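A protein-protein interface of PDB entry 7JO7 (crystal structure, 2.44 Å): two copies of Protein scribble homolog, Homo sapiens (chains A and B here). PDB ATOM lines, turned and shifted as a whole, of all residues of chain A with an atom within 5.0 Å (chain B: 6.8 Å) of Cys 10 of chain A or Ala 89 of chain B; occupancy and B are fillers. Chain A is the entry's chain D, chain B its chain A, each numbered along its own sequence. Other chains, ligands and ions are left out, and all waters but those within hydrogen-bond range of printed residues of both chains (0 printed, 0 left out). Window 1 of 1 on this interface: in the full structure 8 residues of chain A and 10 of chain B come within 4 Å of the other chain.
Among the printed residues, pairs that only touch across the chains: Val 8 of chain A with Ala 89 of chain B, Cys 10 of chain A with Leu 11 of chain B, Cys 10 of chain A with Ala 89 of chain B, Leu 11 of chain A with Thr 87 of chain B, Ala 12 of chain A with Thr 87 of chain B and Ala 89 of chain A with Cys 10 of chain B.
N of Leu 11 of chain B lies within hydrogen-bond range of O of Ile 88 of chain B.
The side-chain amide oxygen of Asn 65 of chain B lies within hydrogen-bond range of the backbone NH of Ala 89 of chain B (2.8 Å).
The backbone carbonyl oxygen (O) of Leu 11 of chain A sits at hydrogen-bond distance from the backbone NH (N) of Ile 88 of chain A.
Cys 10 of chain A touches its own counterpart, Cys 10 of chain B.
Cys 10 of chain A touches Leu 11 of chain B, but with the chains exchanged Leu 11 of chain A does not touch Cys 10 of chain B (4.004 Å).
Cys 10 of chain A touches Ile 88 of chain B, but with the chains exchanged Ile 88 of chain A does not touch Cys 10 of chain B (4.3 Å).
Cys 10 of chain A touches Ala 89 of chain B, and with the chains exchanged Ala 89 of chain A touches Cys 10 of chain B.
Positions printed for both chains: 8, 9, 10, 11, 12, 88 and 89.
The side-chain sulfur (SG) of Cys 10 of chain B forms a disulfide with the side-chain sulfur (SG) of Cys 10 of chain A, 2.0 Å away.
The side-chain hydroxyl (OG1) of Thr 87 of chain B sits at hydrogen-bond distance from the backbone carbonyl oxygen (O) of Cys 10 of chain A, 2.9 Å away.
SG of Cys 10 of chain A lies close to O of Ile 88 of chain B, 3.6 Å away.
Printed residues of chain B within 4 Å of Val 8 of chain A: Ala 89.
Cys 10 of chain A touches just these residues of chain B: Cys 10, Leu 11, Thr 87, Ile 88 and Ala 89.
Printed residues of chain B within 4 Å of Ala 12 of chain A: Thr 87.
Of the printed residues of chain B, Ala 89 of chain A touches Cys 10.
Of the printed residues of chain A, Cys 10 of chain B touches Cys 10 (2.0 Å) and Ala 89 (3.9 Å).
Printed residues of chain A within 4 Å of Ile 88 of chain B: Cys 10.
Printed residues of chain A within 4 Å of Ala 89 of chain B: Val 8 (3.999 Å) and Cys 10 (3.7 Å).
Leu 90 of chain B touches none of the printed residues of chain A.
Leu 91 of chain B touches none of the printed residues of chain A.
Of the 8 printed residues of chain A, 5 touch a printed residue of chain B.
Hydrophobic or aromatic side chains of chain A that line the printed part of chain B: Val 8, Ala 12 and Ala 89.
Hydrophobic or aromatic side chains of chain B that line the printed part of chain A: Ala 89.
Among the printed residues, no Asp or Glu carboxylate lies within 4 Å of a Lys or Arg side-chain nitrogen of the other chain.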
ATOM      1  N   VAL A   8       0.243 -29.155  21.960  1.00  0.00           N
ATOM      2  CA  VAL A   8       1.338 -28.252  22.274  1.00  0.00           C
ATOM      3  C   VAL A   8       2.438 -28.432  21.243  1.00  0.00           C
ATOM      4  O   VAL A   8       2.781 -29.561  20.873  1.00  0.00           O
ATOM      5  CB  VAL A   8       1.878 -28.506  23.696  1.00  0.00           C
ATOM      6  CG1 VAL A   8       3.320 -28.028  23.810  1.00  0.00           C
ATOM      7  CG2 VAL A   8       1.006 -27.825  24.737  1.00  0.00           C
ATOM      8  N   ALA A   9       2.988 -27.312  20.779  1.00  0.00           N
ATOM      9  CA  ALA A   9       4.202 -27.281  19.975  1.00  0.00           C
ATOM     10  C   ALA A   9       5.289 -26.612  20.803  1.00  0.00           C
ATOM     11  O   ALA A   9       5.083 -25.507  21.319  1.00  0.00           O
ATOM     12  CB  ALA A   9       3.981 -26.529  18.661  1.00  0.00           C
ATOM     13  N   CYS A  10       6.430 -27.284  20.938  1.00  0.00           N
ATOM     14  CA  CYS A  10       7.542 -26.841  21.780  1.00  0.00           C
ATOM     15  C   CYS A  10       8.785 -26.784  20.898  1.00  0.00           C
ATOM     16  O   CYS A  10       9.407 -27.809  20.617  1.00  0.00           O
ATOM     17  CB  CYS A  10       7.732 -27.794  22.960  1.00  0.00           C
ATOM     18  SG  CYS A  10       9.153 -27.481  24.025  1.00  0.00           S
ATOM     19  N   LEU A  11       9.153 -25.602  20.434  1.00  0.00           N
ATOM     20  CA  LEU A  11      10.206 -25.480  19.441  1.00  0.00           C
ATOM     21  C   LEU A  11      11.446 -24.868  20.078  1.00  0.00           C
ATOM     22  O   LEU A  11      11.348 -23.952  20.905  1.00  0.00           O
ATOM     23  CB  LEU A  11       9.745 -24.622  18.232  1.00  0.00           C
ATOM     24  CG  LEU A  11       8.298 -24.560  17.695  1.00  0.00           C
ATOM     25  CD1 LEU A  11       8.420 -24.425  16.191  1.00  0.00           C
ATOM     26  CD2 LEU A  11       7.572 -25.804  18.039  1.00  0.00           C
ATOM     27  N   ALA A  12      12.607 -25.373  19.666  1.00  0.00           N
ATOM     28  CA  ALA A  12      13.882 -24.777  20.032  1.00  0.00           C
ATOM     29  C   ALA A  12      14.083 -23.480  19.259  1.00  0.00           C
ATOM     30  O   ALA A  12      13.861 -23.425  18.045  1.00  0.00           O
ATOM     31  CB  ALA A  12      15.012 -25.758  19.739  1.00  0.00           C
ATOM     32  N   THR A  54       4.871 -30.785  14.345  1.00  0.00           N
ATOM     33  CA  THR A  54       3.792 -30.440  15.257  1.00  0.00           C
ATOM     34  C   THR A  54       3.076 -29.155  14.865  1.00  0.00           C
ATOM     35  O   THR A  54       2.148 -28.744  15.565  1.00  0.00           O
ATOM     36  CB  THR A  54       4.325 -30.300  16.685  1.00  0.00           C
ATOM     37  OG1 THR A  54       5.262 -29.215  16.740  1.00  0.00           O
ATOM     38  CG2 THR A  54       5.002 -31.598  17.121  1.00  0.00           C
ATOM     39  N   ILE A  88       9.902 -21.677  22.102  1.00  0.00           N
ATOM     40  CA  ILE A  88       8.630 -21.048  21.767  1.00  0.00           C
ATOM     41  C   ILE A  88       7.559 -22.108  21.982  1.00  0.00           C
ATOM     42  O   ILE A  88       7.511 -23.101  21.246  1.00  0.00           O
ATOM     43  CB  ILE A  88       8.593 -20.526  20.323  1.00  0.00           C
ATOM     44  CG1 ILE A  88       9.655 -19.446  20.126  1.00  0.00           C
ATOM     45  CG2 ILE A  88       7.216 -19.987  19.990  1.00  0.00           C
ATOM     46  CD1 ILE A  88       9.804 -18.994  18.689  1.00  0.00           C
ATOM     47  N   ALA A  89       6.701 -21.903  22.979  1.00  0.00           N
ATOM     48  CA  ALA A  89       5.596 -22.810  23.262  1.00  0.00           C
ATOM     49  C   ALA A  89       4.326 -22.277  22.610  1.00  0.00           C
ATOM     50  O   ALA A  89       3.978 -21.104  22.780  1.00  0.00           O
ATOM     51  CB  ALA A  89       5.390 -22.971  24.768  1.00  0.00           C
ATOM     52  N   VAL B   8       2.084 -25.443  31.272  1.00  0.00           N
ATOM     53  CA  VAL B   8       2.863 -26.002  30.175  1.00  0.00           C
ATOM     54  C   VAL B   8       4.313 -25.577  30.366  1.00  0.00           C
ATOM     55  O   VAL B   8       4.587 -24.429  30.731  1.00  0.00           O
ATOM     56  CB  VAL B   8       2.325 -25.546  28.805  1.00  0.00           C
ATOM     57  CG1 VAL B   8       3.384 -25.745  27.737  1.00  0.00           C
ATOM     58  CG2 VAL B   8       1.064 -26.306  28.444  1.00  0.00           C
ATOM     59  N   ALA B   9       5.236 -26.510  30.136  1.00  0.00           N
ATOM     60  CA  ALA B   9       6.666 -26.248  30.244  1.00  0.00           C
ATOM     61  C   ALA B   9       7.354 -26.735  28.981  1.00  0.00           C
ATOM     62  O   ALA B   9       7.162 -27.882  28.565  1.00  0.00           O
ATOM     63  CB  ALA B   9       7.282 -26.939  31.460  1.00  0.00           C
ATOM     64  N   CYS B  10       8.171 -25.870  28.391  1.00  0.00           N
ATOM     65  CA  CYS B  10       8.866 -26.158  27.143  1.00  0.00           C
ATOM     66  C   CYS B  10      10.335 -25.825  27.350  1.00  0.00           C
ATOM     67  O   CYS B  10      10.691 -24.662  27.577  1.00  0.00           O
ATOM     68  CB  CYS B  10       8.253 -25.360  25.992  1.00  0.00           C
ATOM     69  SG  CYS B  10       9.115 -25.495  24.436  1.00  0.00           S
ATOM     70  N   LEU B  11      11.183 -26.842  27.285  1.00  0.00           N
ATOM     71  CA  LEU B  11      12.599 -26.703  27.583  1.00  0.00           C
ATOM     72  C   LEU B  11      13.439 -27.134  26.391  1.00  0.00           C
ATOM     73  O   LEU B  11      13.132 -28.133  25.729  1.00  0.00           O
ATOM     74  CB  LEU B  11      12.984 -27.543  28.806  1.00  0.00           C
ATOM     75  CG  LEU B  11      12.221 -27.288  30.107  1.00  0.00           C
ATOM     76  CD1 LEU B  11      12.571 -28.360  31.130  1.00  0.00           C
ATOM     77  CD2 LEU B  11      12.535 -25.901  30.639  1.00  0.00           C
ATOM     78  N   ALA B  12      14.511 -26.387  26.140  1.00  0.00           N
ATOM     79  CA  ALA B  12      15.501 -26.760  25.136  1.00  0.00           C
ATOM     80  C   ALA B  12      16.504 -27.722  25.763  1.00  0.00           C
ATOM     81  O   ALA B  12      17.197 -27.364  26.722  1.00  0.00           O
ATOM     82  CB  ALA B  12      16.210 -25.523  24.592  1.00  0.00           C
ATOM     83  N   SER B  63       1.575 -35.132  31.488  1.00  0.00           N
ATOM     84  CA  SER B  63       1.856 -35.606  30.142  1.00  0.00           C
ATOM     85  C   SER B  63       3.260 -35.182  29.748  1.00  0.00           C
ATOM     86  O   SER B  63       3.779 -34.172  30.232  1.00  0.00           O
ATOM     87  CB  SER B  63       0.838 -35.058  29.136  1.00  0.00           C
ATOM     88  OG  SER B  63       1.142 -35.488  27.823  1.00  0.00           O
ATOM     89  N   ILE B  64       3.872 -35.968  28.868  1.00  0.00           N
ATOM     90  CA  ILE B  64       5.211 -35.699  28.361  1.00  0.00           C
ATOM     91  C   ILE B  64       5.165 -35.866  26.851  1.00  0.00           C
ATOM     92  O   ILE B  64       4.809 -36.944  26.357  1.00  0.00           O
ATOM     93  CB  ILE B  64       6.266 -36.628  28.979  1.00  0.00           C
ATOM     94  CG1 ILE B  64       6.197 -36.565  30.505  1.00  0.00           C
ATOM     95  CG2 ILE B  64       7.660 -36.243  28.502  1.00  0.00           C
ATOM     96  CD1 ILE B  64       7.196 -37.459  31.193  1.00  0.00           C
ATOM     97  N   ASN B  65       5.520 -34.806  26.125  1.00  0.00           N
ATOM     98  CA  ASN B  65       5.483 -34.788  24.664  1.00  0.00           C
ATOM     99  C   ASN B  65       4.209 -35.446  24.148  1.00  0.00           C
ATOM    100  O   ASN B  65       4.230 -36.390  23.356  1.00  0.00           O
ATOM    101  CB  ASN B  65       6.724 -35.453  24.080  1.00  0.00           C
ATOM    102  CG  ASN B  65       7.973 -34.611  24.252  1.00  0.00           C
ATOM    103  OD1 ASN B  65       7.932 -33.520  24.815  1.00  0.00           O
ATOM    104  ND2 ASN B  65       9.093 -35.121  23.775  1.00  0.00           N
ATOM    105  N   GLY B  66       3.077 -34.942  24.635  1.00  0.00           N
ATOM    106  CA  GLY B  66       1.780 -35.426  24.218  1.00  0.00           C
ATOM    107  C   GLY B  66       1.377 -36.777  24.763  1.00  0.00           C
ATOM    108  O   GLY B  66       0.238 -37.199  24.529  1.00  0.00           O
ATOM    109  N   LEU B  81      11.384 -38.985  28.880  1.00  0.00           N
ATOM    110  CA  LEU B  81      12.371 -37.939  29.130  1.00  0.00           C
ATOM    111  C   LEU B  81      13.704 -38.265  28.468  1.00  0.00           C
ATOM    112  O   LEU B  81      14.348 -37.387  27.885  1.00  0.00           O
ATOM    113  CB  LEU B  81      12.586 -37.746  30.631  1.00  0.00           C
ATOM    114  CG  LEU B  81      11.390 -37.421  31.520  1.00  0.00           C
ATOM    115  CD1 LEU B  81      11.865 -37.015  32.919  1.00  0.00           C
ATOM    116  CD2 LEU B  81      10.552 -36.333  30.897  1.00  0.00           C
ATOM    117  N   PRO B  86      15.164 -32.663  20.556  1.00  0.00           N
ATOM    118  CA  PRO B  86      15.622 -31.271  20.691  1.00  0.00           C
ATOM    119  C   PRO B  86      14.916 -30.529  21.806  1.00  0.00           C
ATOM    120  O   PRO B  86      15.521 -29.655  22.438  1.00  0.00           O
ATOM    121  CB  PRO B  86      15.325 -30.657  19.312  1.00  0.00           C
ATOM    122  CG  PRO B  86      14.336 -31.578  18.667  1.00  0.00           C
ATOM    123  CD  PRO B  86      14.619 -32.944  19.216  1.00  0.00           C
ATOM    124  N   THR B  87      13.661 -30.863  22.089  1.00  0.00           N
ATOM    125  CA  THR B  87      12.902 -30.203  23.137  1.00  0.00           C
ATOM    126  C   THR B  87      12.170 -31.231  23.990  1.00  0.00           C
ATOM    127  O   THR B  87      12.048 -32.405  23.637  1.00  0.00           O
ATOM    128  CB  THR B  87      11.880 -29.223  22.556  1.00  0.00           C
ATOM    129  OG1 THR B  87      11.009 -29.940  21.678  1.00  0.00           O
ATOM    130  CG2 THR B  87      12.564 -28.086  21.797  1.00  0.00           C
ATOM    131  N   ILE B  88      11.676 -30.759  25.129  1.00  0.00           N
ATOM    132  CA  ILE B  88      10.820 -31.541  26.010  1.00  0.00           C
ATOM    133  C   ILE B  88       9.672 -30.634  26.429  1.00  0.00           C
ATOM    134  O   ILE B  88       9.907 -29.524  26.925  1.00  0.00           O
ATOM    135  CB  ILE B  88      11.582 -32.083  27.230  1.00  0.00           C
ATOM    136  CG1 ILE B  88      10.624 -32.810  28.170  1.00  0.00           C
ATOM    137  CG2 ILE B  88      12.285 -30.971  27.974  1.00  0.00           C
ATOM    138  CD1 ILE B  88       9.977 -34.015  27.542  1.00  0.00           C
ATOM    139  N   ALA B  89       8.443 -31.079  26.191  1.00  0.00           N
ATOM    140  CA  ALA B  89       7.241 -30.341  26.554  1.00  0.00           C
ATOM    141  C   ALA B  89       6.556 -31.063  27.705  1.00  0.00           C
ATOM    142  O   ALA B  89       6.274 -32.261  27.610  1.00  0.00           O
ATOM    143  CB  ALA B  89       6.288 -30.213  25.361  1.00  0.00           C
ATOM    144  N   LEU B  90       6.296 -30.343  28.791  1.00  0.00           N
ATOM    145  CA  LEU B  90       5.672 -30.919  29.972  1.00  0.00           C
ATOM    146  C   LEU B  90       4.377 -30.196  30.300  1.00  0.00           C
ATOM    147  O   LEU B  90       4.283 -28.969  30.161  1.00  0.00           O
ATOM    148  CB  LEU B  90       6.613 -30.857  31.172  1.00  0.00           C
ATOM    149  CG  LEU B  90       7.891 -31.685  31.051  1.00  0.00           C
ATOM    150  CD1 LEU B  90       8.837 -31.360  32.194  1.00  0.00           C
ATOM    151  CD2 LEU B  90       7.547 -33.160  31.035  1.00  0.00           C
ATOM    152  N   LEU B  91       3.377 -30.983  30.722  1.00  0.00           N
ATOM    153  CA  LEU B  91       2.111 -30.485  31.256  1.00  0.00           C
ATOM    154  C   LEU B  91       2.082 -30.854  32.728  1.00  0.00           C
ATOM    155  O   LEU B  91       1.937 -32.028  33.079  1.00  0.00           O
ATOM    156  CB  LEU B  91       0.892 -31.075  30.553  1.00  0.00           C
ATOM    157  CG  LEU B  91      -0.304 -30.164  30.296  1.00  0.00           C
ATOM    158  CD1 LEU B  91      -1.402 -31.035  29.792  1.00  0.00           C
ATOM    159  CD2 LEU B  91      -0.742 -29.476  31.565  1.00  0.00           C
